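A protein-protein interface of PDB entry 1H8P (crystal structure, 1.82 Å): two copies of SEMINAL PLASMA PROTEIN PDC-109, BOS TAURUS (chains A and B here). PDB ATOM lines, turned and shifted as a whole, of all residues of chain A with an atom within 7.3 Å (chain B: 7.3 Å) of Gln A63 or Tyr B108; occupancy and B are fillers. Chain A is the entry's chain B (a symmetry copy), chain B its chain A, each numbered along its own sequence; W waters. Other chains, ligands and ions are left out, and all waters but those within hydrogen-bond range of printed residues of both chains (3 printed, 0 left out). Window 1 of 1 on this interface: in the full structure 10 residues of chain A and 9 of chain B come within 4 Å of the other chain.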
ATOM      1  N   CYS A  38     -17.154  -8.721 -17.645  1.00  0.00           N
ATOM      2  CA  CYS A  38     -17.610  -7.597 -18.446  1.00  0.00           C
ATOM      3  C   CYS A  38     -18.427  -8.229 -19.557  1.00  0.00           C
ATOM      4  O   CYS A  38     -18.146  -9.355 -19.971  1.00  0.00           O
ATOM      5  CB  CYS A  38     -16.407  -6.854 -18.998  1.00  0.00           C
ATOM      6  SG  CYS A  38     -15.473  -6.088 -17.646  1.00  0.00           S
ATOM      7  N   PHE A  45     -19.387  -2.256 -26.729  1.00  0.00           N
ATOM      8  CA  PHE A  45     -18.101  -2.462 -26.077  1.00  0.00           C
ATOM      9  C   PHE A  45     -18.310  -3.048 -24.684  1.00  0.00           C
ATOM     10  O   PHE A  45     -19.277  -2.709 -23.998  1.00  0.00           O
ATOM     11  CB  PHE A  45     -17.348  -1.131 -26.007  1.00  0.00           C
ATOM     12  CG  PHE A  45     -15.894  -1.274 -25.684  1.00  0.00           C
ATOM     13  CD1 PHE A  45     -15.461  -1.309 -24.362  1.00  0.00           C
ATOM     14  CD2 PHE A  45     -14.949  -1.382 -26.705  1.00  0.00           C
ATOM     15  CE1 PHE A  45     -14.104  -1.447 -24.059  1.00  0.00           C
ATOM     16  CE2 PHE A  45     -13.597  -1.521 -26.413  1.00  0.00           C
ATOM     17  CZ  PHE A  45     -13.173  -1.552 -25.089  1.00  0.00           C
ATOM     18  N   PRO A  46     -17.409  -3.951 -24.255  1.00  0.00           N
ATOM     19  CA  PRO A  46     -17.512  -4.586 -22.937  1.00  0.00           C
ATOM     20  C   PRO A  46     -17.651  -3.586 -21.794  1.00  0.00           C
ATOM     21  O   PRO A  46     -16.920  -2.596 -21.726  1.00  0.00           O
ATOM     22  CB  PRO A  46     -16.220  -5.399 -22.844  1.00  0.00           C
ATOM     23  CG  PRO A  46     -15.982  -5.794 -24.272  1.00  0.00           C
ATOM     24  CD  PRO A  46     -16.266  -4.496 -25.009  1.00  0.00           C
ATOM     25  N   CYS A  61     -14.935  -1.592 -19.825  1.00  0.00           N
ATOM     26  CA  CYS A  61     -13.842  -2.315 -19.202  1.00  0.00           C
ATOM     27  C   CYS A  61     -12.479  -2.184 -19.835  1.00  0.00           C
ATOM     28  O   CYS A  61     -12.330  -2.294 -21.049  1.00  0.00           O
ATOM     29  CB  CYS A  61     -14.191  -3.798 -19.125  1.00  0.00           C
ATOM     30  SG  CYS A  61     -15.629  -4.108 -18.072  1.00  0.00           S
ATOM     31  N   ALA A  62     -11.488  -1.953 -18.979  1.00  0.00           N
ATOM     32  CA  ALA A  62     -10.094  -1.877 -19.381  1.00  0.00           C
ATOM     33  C   ALA A  62      -9.593  -3.297 -19.117  1.00  0.00           C
ATOM     34  O   ALA A  62     -10.297  -4.100 -18.497  1.00  0.00           O
ATOM     35  CB  ALA A  62      -9.341  -0.879 -18.515  1.00  0.00           C
ATOM     36  N   GLN A  63      -8.386  -3.613 -19.568  1.00  0.00           N
ATOM     37  CA  GLN A  63      -7.851  -4.955 -19.381  1.00  0.00           C
ATOM     38  C   GLN A  63      -7.918  -5.435 -17.930  1.00  0.00           C
ATOM     39  O   GLN A  63      -8.288  -6.584 -17.664  1.00  0.00           O
ATOM     40  CB  GLN A  63      -6.407  -5.014 -19.885  1.00  0.00           C
ATOM     41  CG  GLN A  63      -5.855  -6.420 -20.029  1.00  0.00           C
ATOM     42  CD  GLN A  63      -4.508  -6.440 -20.721  1.00  0.00           C
ATOM     43  OE1 GLN A  63      -4.372  -5.972 -21.852  1.00  0.00           O
ATOM     44  NE2 GLN A  63      -3.501  -6.980 -20.043  1.00  0.00           N
ATOM     45  N   ARG A  64      -7.578  -4.559 -16.994  1.00  0.00           N
ATOM     46  CA  ARG A  64      -7.581  -4.918 -15.576  1.00  0.00           C
ATOM     47  C   ARG A  64      -8.973  -5.199 -15.015  1.00  0.00           C
ATOM     48  O   ARG A  64      -9.111  -5.858 -13.983  1.00  0.00           O
ATOM     49  CB  ARG A  64      -6.934  -3.806 -14.749  1.00  0.00           C
ATOM     50  CG  ARG A  64      -7.846  -2.608 -14.525  1.00  0.00           C
ATOM     51  CD  ARG A  64      -7.189  -1.550 -13.654  1.00  0.00           C
ATOM     52  NE  ARG A  64      -8.162  -0.555 -13.211  1.00  0.00           N
ATOM     53  CZ  ARG A  64      -9.103  -0.783 -12.297  1.00  0.00           C
ATOM     54  NH1 ARG A  64      -9.196  -1.973 -11.721  1.00  0.00           N
ATOM     55  NH2 ARG A  64      -9.955   0.178 -11.967  1.00  0.00           N
ATOM     56  N   ASP A  65     -10.003  -4.702 -15.694  1.00  0.00           N
ATOM     57  CA  ASP A  65     -11.374  -4.877 -15.228  1.00  0.00           C
ATOM     58  C   ASP A  65     -12.002  -6.232 -15.512  1.00  0.00           C
ATOM     59  O   ASP A  65     -12.928  -6.634 -14.815  1.00  0.00           O
ATOM     60  CB  ASP A  65     -12.275  -3.789 -15.818  1.00  0.00           C
ATOM     61  CG  ASP A  65     -11.853  -2.397 -15.398  1.00  0.00           C
ATOM     62  OD1 ASP A  65     -11.686  -2.171 -14.182  1.00  0.00           O
ATOM     63  OD2 ASP A  65     -11.694  -1.531 -16.282  1.00  0.00           O
ATOM     64  N   TYR A  66     -11.522  -6.933 -16.538  1.00  0.00           N
ATOM     65  CA  TYR A  66     -12.097  -8.235 -16.856  1.00  0.00           C
ATOM     66  C   TYR A  66     -11.951  -9.201 -15.693  1.00  0.00           C
ATOM     67  O   TYR A  66     -10.984  -9.140 -14.934  1.00  0.00           O
ATOM     68  CB  TYR A  66     -11.456  -8.825 -18.113  1.00  0.00           C
ATOM     69  CG  TYR A  66     -11.835  -8.067 -19.362  1.00  0.00           C
ATOM     70  CD1 TYR A  66     -11.079  -6.982 -19.794  1.00  0.00           C
ATOM     71  CD2 TYR A  66     -12.982  -8.401 -20.080  1.00  0.00           C
ATOM     72  CE1 TYR A  66     -11.459  -6.239 -20.915  1.00  0.00           C
ATOM     73  CE2 TYR A  66     -13.369  -7.669 -21.200  1.00  0.00           C
ATOM     74  CZ  TYR A  66     -12.605  -6.591 -21.611  1.00  0.00           C
ATOM     75  OH  TYR A  66     -12.987  -5.860 -22.712  1.00  0.00           O
ATOM     76  N   ALA A  67     -12.926 -10.089 -15.558  1.00  0.00           N
ATOM     77  CA  ALA A  67     -12.925 -11.057 -14.473  1.00  0.00           C
ATOM     78  C   ALA A  67     -11.700 -11.947 -14.516  1.00  0.00           C
ATOM     79  O   ALA A  67     -11.308 -12.437 -15.573  1.00  0.00           O
ATOM     80  CB  ALA A  67     -14.191 -11.912 -14.535  1.00  0.00           C
ATOM     81  N   LYS A  68     -11.087 -12.143 -13.355  1.00  0.00           N
ATOM     82  CA  LYS A  68      -9.924 -13.001 -13.265  1.00  0.00           C
ATOM     83  C   LYS A  68     -10.371 -14.348 -12.720  1.00  0.00           C
ATOM     84  O   LYS A  68     -11.438 -14.463 -12.114  1.00  0.00           O
ATOM     85  CB  LYS A  68      -8.872 -12.371 -12.352  1.00  0.00           C
ATOM     86  CG  LYS A  68      -8.250 -11.116 -12.956  1.00  0.00           C
ATOM     87  CD  LYS A  68      -7.229 -10.477 -12.037  1.00  0.00           C
ATOM     88  CE  LYS A  68      -6.538  -9.308 -12.724  1.00  0.00           C
ATOM     89  NZ  LYS A  68      -7.500  -8.256 -13.151  1.00  0.00           N
ATOM     90  N   GLN B  63      -3.864 -16.820 -22.445  1.00  0.00           N
ATOM     91  CA  GLN B  63      -3.819 -15.410 -22.063  1.00  0.00           C
ATOM     92  C   GLN B  63      -2.423 -14.783 -22.117  1.00  0.00           C
ATOM     93  O   GLN B  63      -2.256 -13.660 -22.598  1.00  0.00           O
ATOM     94  CB  GLN B  63      -4.406 -15.240 -20.654  1.00  0.00           C
ATOM     95  CG  GLN B  63      -4.379 -13.813 -20.103  1.00  0.00           C
ATOM     96  CD  GLN B  63      -3.047 -13.439 -19.463  1.00  0.00           C
ATOM     97  OE1 GLN B  63      -2.576 -14.110 -18.541  1.00  0.00           O
ATOM     98  NE2 GLN B  63      -2.439 -12.359 -19.945  1.00  0.00           N
ATOM     99  N   ALA B  67       0.178 -10.448 -27.488  1.00  0.00           N
ATOM    100  CA  ALA B  67       1.184  -9.403 -27.550  1.00  0.00           C
ATOM    101  C   ALA B  67       0.986  -8.356 -26.462  1.00  0.00           C
ATOM    102  O   ALA B  67      -0.141  -8.085 -26.036  1.00  0.00           O
ATOM    103  CB  ALA B  67       1.162  -8.740 -28.927  1.00  0.00           C
ATOM    104  N   LYS B  68       2.098  -7.789 -26.008  1.00  0.00           N
ATOM    105  CA  LYS B  68       2.082  -6.746 -24.992  1.00  0.00           C
ATOM    106  C   LYS B  68       2.340  -5.410 -25.666  1.00  0.00           C
ATOM    107  O   LYS B  68       2.856  -5.354 -26.784  1.00  0.00           O
ATOM    108  CB  LYS B  68       3.169  -6.984 -23.938  1.00  0.00           C
ATOM    109  CG  LYS B  68       2.771  -7.918 -22.809  1.00  0.00           C
ATOM    110  CD  LYS B  68       2.516  -9.318 -23.310  1.00  0.00           C
ATOM    111  CE  LYS B  68       2.298 -10.277 -22.152  1.00  0.00           C
ATOM    112  NZ  LYS B  68       2.158 -11.676 -22.634  1.00  0.00           N
ATOM    113  N   CYS B  69       1.979  -4.336 -24.978  1.00  0.00           N
ATOM    114  CA  CYS B  69       2.187  -2.990 -25.486  1.00  0.00           C
ATOM    115  C   CYS B  69       3.652  -2.755 -25.810  1.00  0.00           C
ATOM    116  O   CYS B  69       4.539  -3.293 -25.150  1.00  0.00           O
ATOM    117  CB  CYS B  69       1.770  -1.957 -24.444  1.00  0.00           C
ATOM    118  SG  CYS B  69      -0.010  -1.828 -24.108  1.00  0.00           S
ATOM    119  N   CYS B  83      -0.298   4.140 -22.549  1.00  0.00           N
ATOM    120  CA  CYS B  83      -1.524   3.929 -23.298  1.00  0.00           C
ATOM    121  C   CYS B  83      -2.193   5.286 -23.424  1.00  0.00           C
ATOM    122  O   CYS B  83      -1.921   6.197 -22.640  1.00  0.00           O
ATOM    123  CB  CYS B  83      -2.441   2.979 -22.541  1.00  0.00           C
ATOM    124  SG  CYS B  83      -1.748   1.312 -22.343  1.00  0.00           S
ATOM    125  N   THR B  84      -3.068   5.431 -24.409  1.00  0.00           N
ATOM    126  CA  THR B  84      -3.751   6.703 -24.592  1.00  0.00           C
ATOM    127  C   THR B  84      -5.197   6.475 -25.008  1.00  0.00           C
ATOM    128  O   THR B  84      -5.510   5.477 -25.653  1.00  0.00           O
ATOM    129  CB  THR B  84      -3.047   7.568 -25.671  1.00  0.00           C
ATOM    130  OG1 THR B  84      -3.712   8.833 -25.779  1.00  0.00           O
ATOM    131  CG2 THR B  84      -3.077   6.867 -27.029  1.00  0.00           C
ATOM    132  N   SER B  88      -9.446   6.748 -29.752  1.00  0.00           N
ATOM    133  CA  SER B  88     -10.350   5.629 -29.517  1.00  0.00           C
ATOM    134  C   SER B  88     -11.739   6.072 -29.089  1.00  0.00           C
ATOM    135  O   SER B  88     -11.895   6.981 -28.273  1.00  0.00           O
ATOM    136  CB  SER B  88      -9.785   4.691 -28.448  1.00  0.00           C
ATOM    137  OG  SER B  88     -10.736   3.688 -28.142  1.00  0.00           O
ATOM    138  N   MET B  89     -12.750   5.412 -29.637  1.00  0.00           N
ATOM    139  CA  MET B  89     -14.128   5.729 -29.302  1.00  0.00           C
ATOM    140  C   MET B  89     -14.521   5.131 -27.959  1.00  0.00           C
ATOM    141  O   MET B  89     -15.536   5.521 -27.386  1.00  0.00           O
ATOM    142  CB  MET B  89     -15.079   5.167 -30.361  1.00  0.00           C
ATOM    143  CG  MET B  89     -15.002   5.818 -31.728  1.00  0.00           C
ATOM    144  SD  MET B  89     -16.137   4.993 -32.873  1.00  0.00           S
ATOM    145  CE  MET B  89     -17.714   5.275 -32.057  1.00  0.00           C
ATOM    146  N   TRP B  90     -13.716   4.204 -27.442  1.00  0.00           N
ATOM    147  CA  TRP B  90     -14.091   3.535 -26.201  1.00  0.00           C
ATOM    148  C   TRP B  90     -13.106   3.378 -25.057  1.00  0.00           C
ATOM    149  O   TRP B  90     -13.462   3.565 -23.895  1.00  0.00           O
ATOM    150  CB  TRP B  90     -14.578   2.114 -26.504  1.00  0.00           C
ATOM    151  CG  TRP B  90     -15.415   1.960 -27.729  1.00  0.00           C
ATOM    152  CD1 TRP B  90     -14.980   1.686 -28.993  1.00  0.00           C
ATOM    153  CD2 TRP B  90     -16.836   2.054 -27.801  1.00  0.00           C
ATOM    154  NE1 TRP B  90     -16.051   1.598 -29.853  1.00  0.00           N
ATOM    155  CE2 TRP B  90     -17.202   1.822 -29.146  1.00  0.00           C
ATOM    156  CE3 TRP B  90     -17.840   2.313 -26.858  1.00  0.00           C
ATOM    157  CZ2 TRP B  90     -18.531   1.841 -29.572  1.00  0.00           C
ATOM    158  CZ3 TRP B  90     -19.165   2.331 -27.284  1.00  0.00           C
ATOM    159  CH2 TRP B  90     -19.497   2.096 -28.629  1.00  0.00           C
ATOM    160  N   MET B  91     -11.875   3.014 -25.379  1.00  0.00           N
ATOM    161  CA  MET B  91     -10.920   2.699 -24.330  1.00  0.00           C
ATOM    162  C   MET B  91      -9.478   3.073 -24.648  1.00  0.00           C
ATOM    163  O   MET B  91      -9.107   3.222 -25.811  1.00  0.00           O
ATOM    164  CB  MET B  91     -11.037   1.188 -24.091  1.00  0.00           C
ATOM    165  CG  MET B  91     -10.102   0.567 -23.078  1.00  0.00           C
ATOM    166  SD  MET B  91     -10.439   1.175 -21.449  1.00  0.00           S
ATOM    167  CE  MET B  91     -12.237   0.962 -21.340  1.00  0.00           C
ATOM    168  N   SER B  92      -8.667   3.220 -23.602  1.00  0.00           N
ATOM    169  CA  SER B  92      -7.257   3.540 -23.780  1.00  0.00           C
ATOM    170  C   SER B  92      -6.629   2.365 -24.509  1.00  0.00           C
ATOM    171  O   SER B  92      -7.016   1.213 -24.294  1.00  0.00           O
ATOM    172  CB  SER B  92      -6.568   3.728 -22.425  1.00  0.00           C
ATOM    173  OG  SER B  92      -7.185   4.769 -21.692  1.00  0.00           O
ATOM    174  N   TRP B  93      -5.652   2.654 -25.359  1.00  0.00           N
ATOM    175  CA  TRP B  93      -4.994   1.619 -26.138  1.00  0.00           C
ATOM    176  C   TRP B  93      -3.507   1.900 -26.304  1.00  0.00           C
ATOM    177  O   TRP B  93      -3.010   2.963 -25.925  1.00  0.00           O
ATOM    178  CB  TRP B  93      -5.638   1.534 -27.522  1.00  0.00           C
ATOM    179  CG  TRP B  93      -5.489   2.812 -28.296  1.00  0.00           C
ATOM    180  CD1 TRP B  93      -6.236   3.947 -28.160  1.00  0.00           C
ATOM    181  CD2 TRP B  93      -4.481   3.106 -29.265  1.00  0.00           C
ATOM    182  NE1 TRP B  93      -5.749   4.936 -28.987  1.00  0.00           N
ATOM    183  CE2 TRP B  93      -4.671   4.445 -29.675  1.00  0.00           C
ATOM    184  CE3 TRP B  93      -3.431   2.369 -29.827  1.00  0.00           C
ATOM    185  CZ2 TRP B  93      -3.847   5.065 -30.626  1.00  0.00           C
ATOM    186  CZ3 TRP B  93      -2.610   2.986 -30.776  1.00  0.00           C
ATOM    187  CH2 TRP B  93      -2.826   4.320 -31.163  1.00  0.00           C
ATOM    188  N   CYS B  94      -2.804   0.932 -26.877  1.00  0.00           N
ATOM    189  CA  CYS B  94      -1.380   1.068 -27.119  1.00  0.00           C
ATOM    190  C   CYS B  94      -1.026   0.342 -28.404  1.00  0.00           C
ATOM    191  O   CYS B  94      -1.737  -0.566 -28.836  1.00  0.00           O
ATOM    192  CB  CYS B  94      -0.592   0.454 -25.976  1.00  0.00           C
ATOM    193  SG  CYS B  94      -0.785  -1.355 -25.918  1.00  0.00           S
ATOM    194  N   LEU B  96       1.214  -2.107 -30.902  1.00  0.00           N
ATOM    195  CA  LEU B  96       1.873  -3.402 -30.766  1.00  0.00           C
ATOM    196  C   LEU B  96       3.174  -3.396 -31.568  1.00  0.00           C
ATOM    197  O   LEU B  96       3.735  -4.449 -31.876  1.00  0.00           O
ATOM    198  CB  LEU B  96       0.957  -4.535 -31.245  1.00  0.00           C
ATOM    199  CG  LEU B  96      -0.263  -4.817 -30.360  1.00  0.00           C
ATOM    200  CD1 LEU B  96      -0.973  -6.078 -30.843  1.00  0.00           C
ATOM    201  CD2 LEU B  96       0.183  -5.000 -28.923  1.00  0.00           C
ATOM    202  N   TRP B 106      -2.452  -2.712 -32.820  1.00  0.00           N
ATOM    203  CA  TRP B 106      -2.730  -2.222 -31.476  1.00  0.00           C
ATOM    204  C   TRP B 106      -3.582  -3.171 -30.647  1.00  0.00           C
ATOM    205  O   TRP B 106      -4.057  -4.200 -31.129  1.00  0.00           O
ATOM    206  CB  TRP B 106      -3.474  -0.889 -31.569  1.00  0.00           C
ATOM    207  CG  TRP B 106      -4.785  -1.013 -32.295  1.00  0.00           C
ATOM    208  CD1 TRP B 106      -4.974  -1.063 -33.648  1.00  0.00           C
ATOM    209  CD2 TRP B 106      -6.087  -1.152 -31.705  1.00  0.00           C
ATOM    210  NE1 TRP B 106      -6.311  -1.226 -33.937  1.00  0.00           N
ATOM    211  CE2 TRP B 106      -7.015  -1.286 -32.763  1.00  0.00           C
ATOM    212  CE3 TRP B 106      -6.558  -1.182 -30.384  1.00  0.00           C
ATOM    213  CZ2 TRP B 106      -8.388  -1.444 -32.541  1.00  0.00           C
ATOM    214  CZ3 TRP B 106      -7.924  -1.341 -30.164  1.00  0.00           C
ATOM    215  CH2 TRP B 106      -8.823  -1.470 -31.239  1.00  0.00           C
ATOM    216  N   LYS B 107      -3.785  -2.791 -29.391  1.00  0.00           N
ATOM    217  CA  LYS B 107      -4.614  -3.561 -28.474  1.00  0.00           C
ATOM    218  C   LYS B 107      -5.115  -2.589 -27.416  1.00  0.00           C
ATOM    219  O   LYS B 107      -4.533  -1.523 -27.227  1.00  0.00           O
ATOM    220  CB  LYS B 107      -3.799  -4.672 -27.806  1.00  0.00           C
ATOM    221  CG  LYS B 107      -2.864  -4.199 -26.702  1.00  0.00           C
ATOM    222  CD  LYS B 107      -2.144  -5.383 -26.065  1.00  0.00           C
ATOM    223  CE  LYS B 107      -1.585  -5.019 -24.708  1.00  0.00           C
ATOM    224  NZ  LYS B 107      -2.676  -4.690 -23.744  1.00  0.00           N
ATOM    225  N   TYR B 108      -6.205  -2.929 -26.740  1.00  0.00           N
ATOM    226  CA  TYR B 108      -6.684  -2.046 -25.688  1.00  0.00           C
ATOM    227  C   TYR B 108      -5.865  -2.324 -24.440  1.00  0.00           C
ATOM    228  O   TYR B 108      -5.281  -3.400 -24.299  1.00  0.00           O
ATOM    229  CB  TYR B 108      -8.159  -2.291 -25.384  1.00  0.00           C
ATOM    230  CG  TYR B 108      -9.085  -1.788 -26.456  1.00  0.00           C
ATOM    231  CD1 TYR B 108      -9.807  -2.676 -27.249  1.00  0.00           C
ATOM    232  CD2 TYR B 108      -9.240  -0.422 -26.682  1.00  0.00           C
ATOM    233  CE1 TYR B 108     -10.665  -2.222 -28.242  1.00  0.00           C
ATOM    234  CE2 TYR B 108     -10.094   0.045 -27.675  1.00  0.00           C
ATOM    235  CZ  TYR B 108     -10.804  -0.863 -28.450  1.00  0.00           C
ATOM    236  OH  TYR B 108     -11.651  -0.423 -29.429  1.00  0.00           O
ATOM    237  N   CYS B 109      -5.819  -1.350 -23.541  1.00  0.00           N
ATOM    238  CA  CYS B 109      -5.085  -1.494 -22.293  1.00  0.00           C
ATOM    239  C   CYS B 109      -6.039  -1.758 -21.134  1.00  0.00           C
ATOM    240  O   CYS B 109      -7.235  -1.979 -21.401  1.00  0.00           O
ATOM    241  CB  CYS B 109      -4.288  -0.228 -22.019  1.00  0.00           C
ATOM    242  SG  CYS B 109      -3.079   0.142 -23.324  1.00  0.00           S
ATOM    243  OXT CYS B 109      -5.578  -1.747 -19.976  1.00  0.00           O
HETATM  244  O   HOH W   1      -8.756  -4.183 -22.493  1.00  0.00           O
HETATM  245  O   HOH W   2      -6.473  -5.883 -24.057  1.00  0.00           O
HETATM  246  O   HOH W   3      -6.058  -2.195 -17.571  1.00  0.00           O
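O of Cys B109 lies within hydrogen-bond range of N of Gln A63 (2.7 Å). The side-chain amino group of Lys B107 is in hydrogen-bond range of the side-chain amide oxygen of Gln A63 (2.8 Å).
The backbone NH of Cys B94 lies close to the side-chain sulfur of Cys B109 (3.7 Å). The backbone carbonyl oxygen (O) of Ser B92 sits at hydrogen-bond distance from the backbone NH (N) of Cys B109. The side-chain sulfur of Cys B83 forms a disulfide with the side-chain sulfur of Cys B109, at 2.0 Å. The backbone NH (N) of Cys B94 is in hydrogen-bond range of the backbone carbonyl oxygen (O) of Lys B107 (3.0 Å). SG of Cys B94 is disulfide-bonded to SG of Cys B69. O of Met B91 is in hydrogen-bond range of OG of Ser B88 (2.9 Å).
Trp B90 touches Phe A45. Met B91 touches Phe A45. CE2 of Phe A45 touches CZ of Tyr B108 (3.5 Å). O of Cys A61 touches CE of Met B91 (3.3 Å). Met B91 touches Ala A62. O of Cys B109 touches CA of Ala A62, at 3.5 Å. Gln A63 touches Tyr B108.
Of the printed residues of chain B, Phe A45 touches Trp B90 (3.5 Å), Met B91 (3.6 Å) and Tyr B108 (3.5 Å). Of the printed residues of chain B, Cys A61 touches Met B91. Gln A63 touches just these residues of chain B: Lys B107 (2.8 Å), Tyr B108 (3.7 Å) and Cys B109 (2.7 Å). Arg A64 touches none of the printed residues of chain B. Tyr A66 touches none of the printed residues of chain B. Printed residues of chain A within 4 Å of Trp B90: Phe A45 (3.5 Å). Of the printed residues of chain A, Met B91 touches Phe A45, Cys A61 and Ala A62. Tyr B108 touches just these residues of chain A: Phe A45 (3.5 Å) and Gln A63 (3.7 Å). Of the printed residues of chain A, Cys B109 touches Ala A62 and Gln A63. The nearest residue of chain A that does not touch Tyr B108 is Cys A61 (6.0 Å).
Hydrophobic or aromatic side chains of chain B within 4 Å of the printed part of chain A: Trp B90, Met B91 and Tyr B108. Among the printed residues, 9 pairs touch across the chains. Among the printed residues, no Asp or Glu carboxylate lies within 4 Å of a Lys or Arg side-chain nitrogen of the other chain.
3 positions are printed for both chains. Of the 9 pairs that touch across the chains among the printed residues, none has its exchanged pair printed and touching as well.
Water W3 lies within hydrogen-bond range of the chain-end carboxylate of Cys B109, the backbone NH of Arg A64 and the backbone NH of Gln A63. Water W2 lies within hydrogen-bond range of the backbone carbonyl oxygen (O) of Tyr B108 (2.8 Å) and the side-chain amide oxygen (OE1) of Gln A63 (3.0 Å). Water W1 lies within hydrogen-bond range of O of Cys B109 and N of Gln A63.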
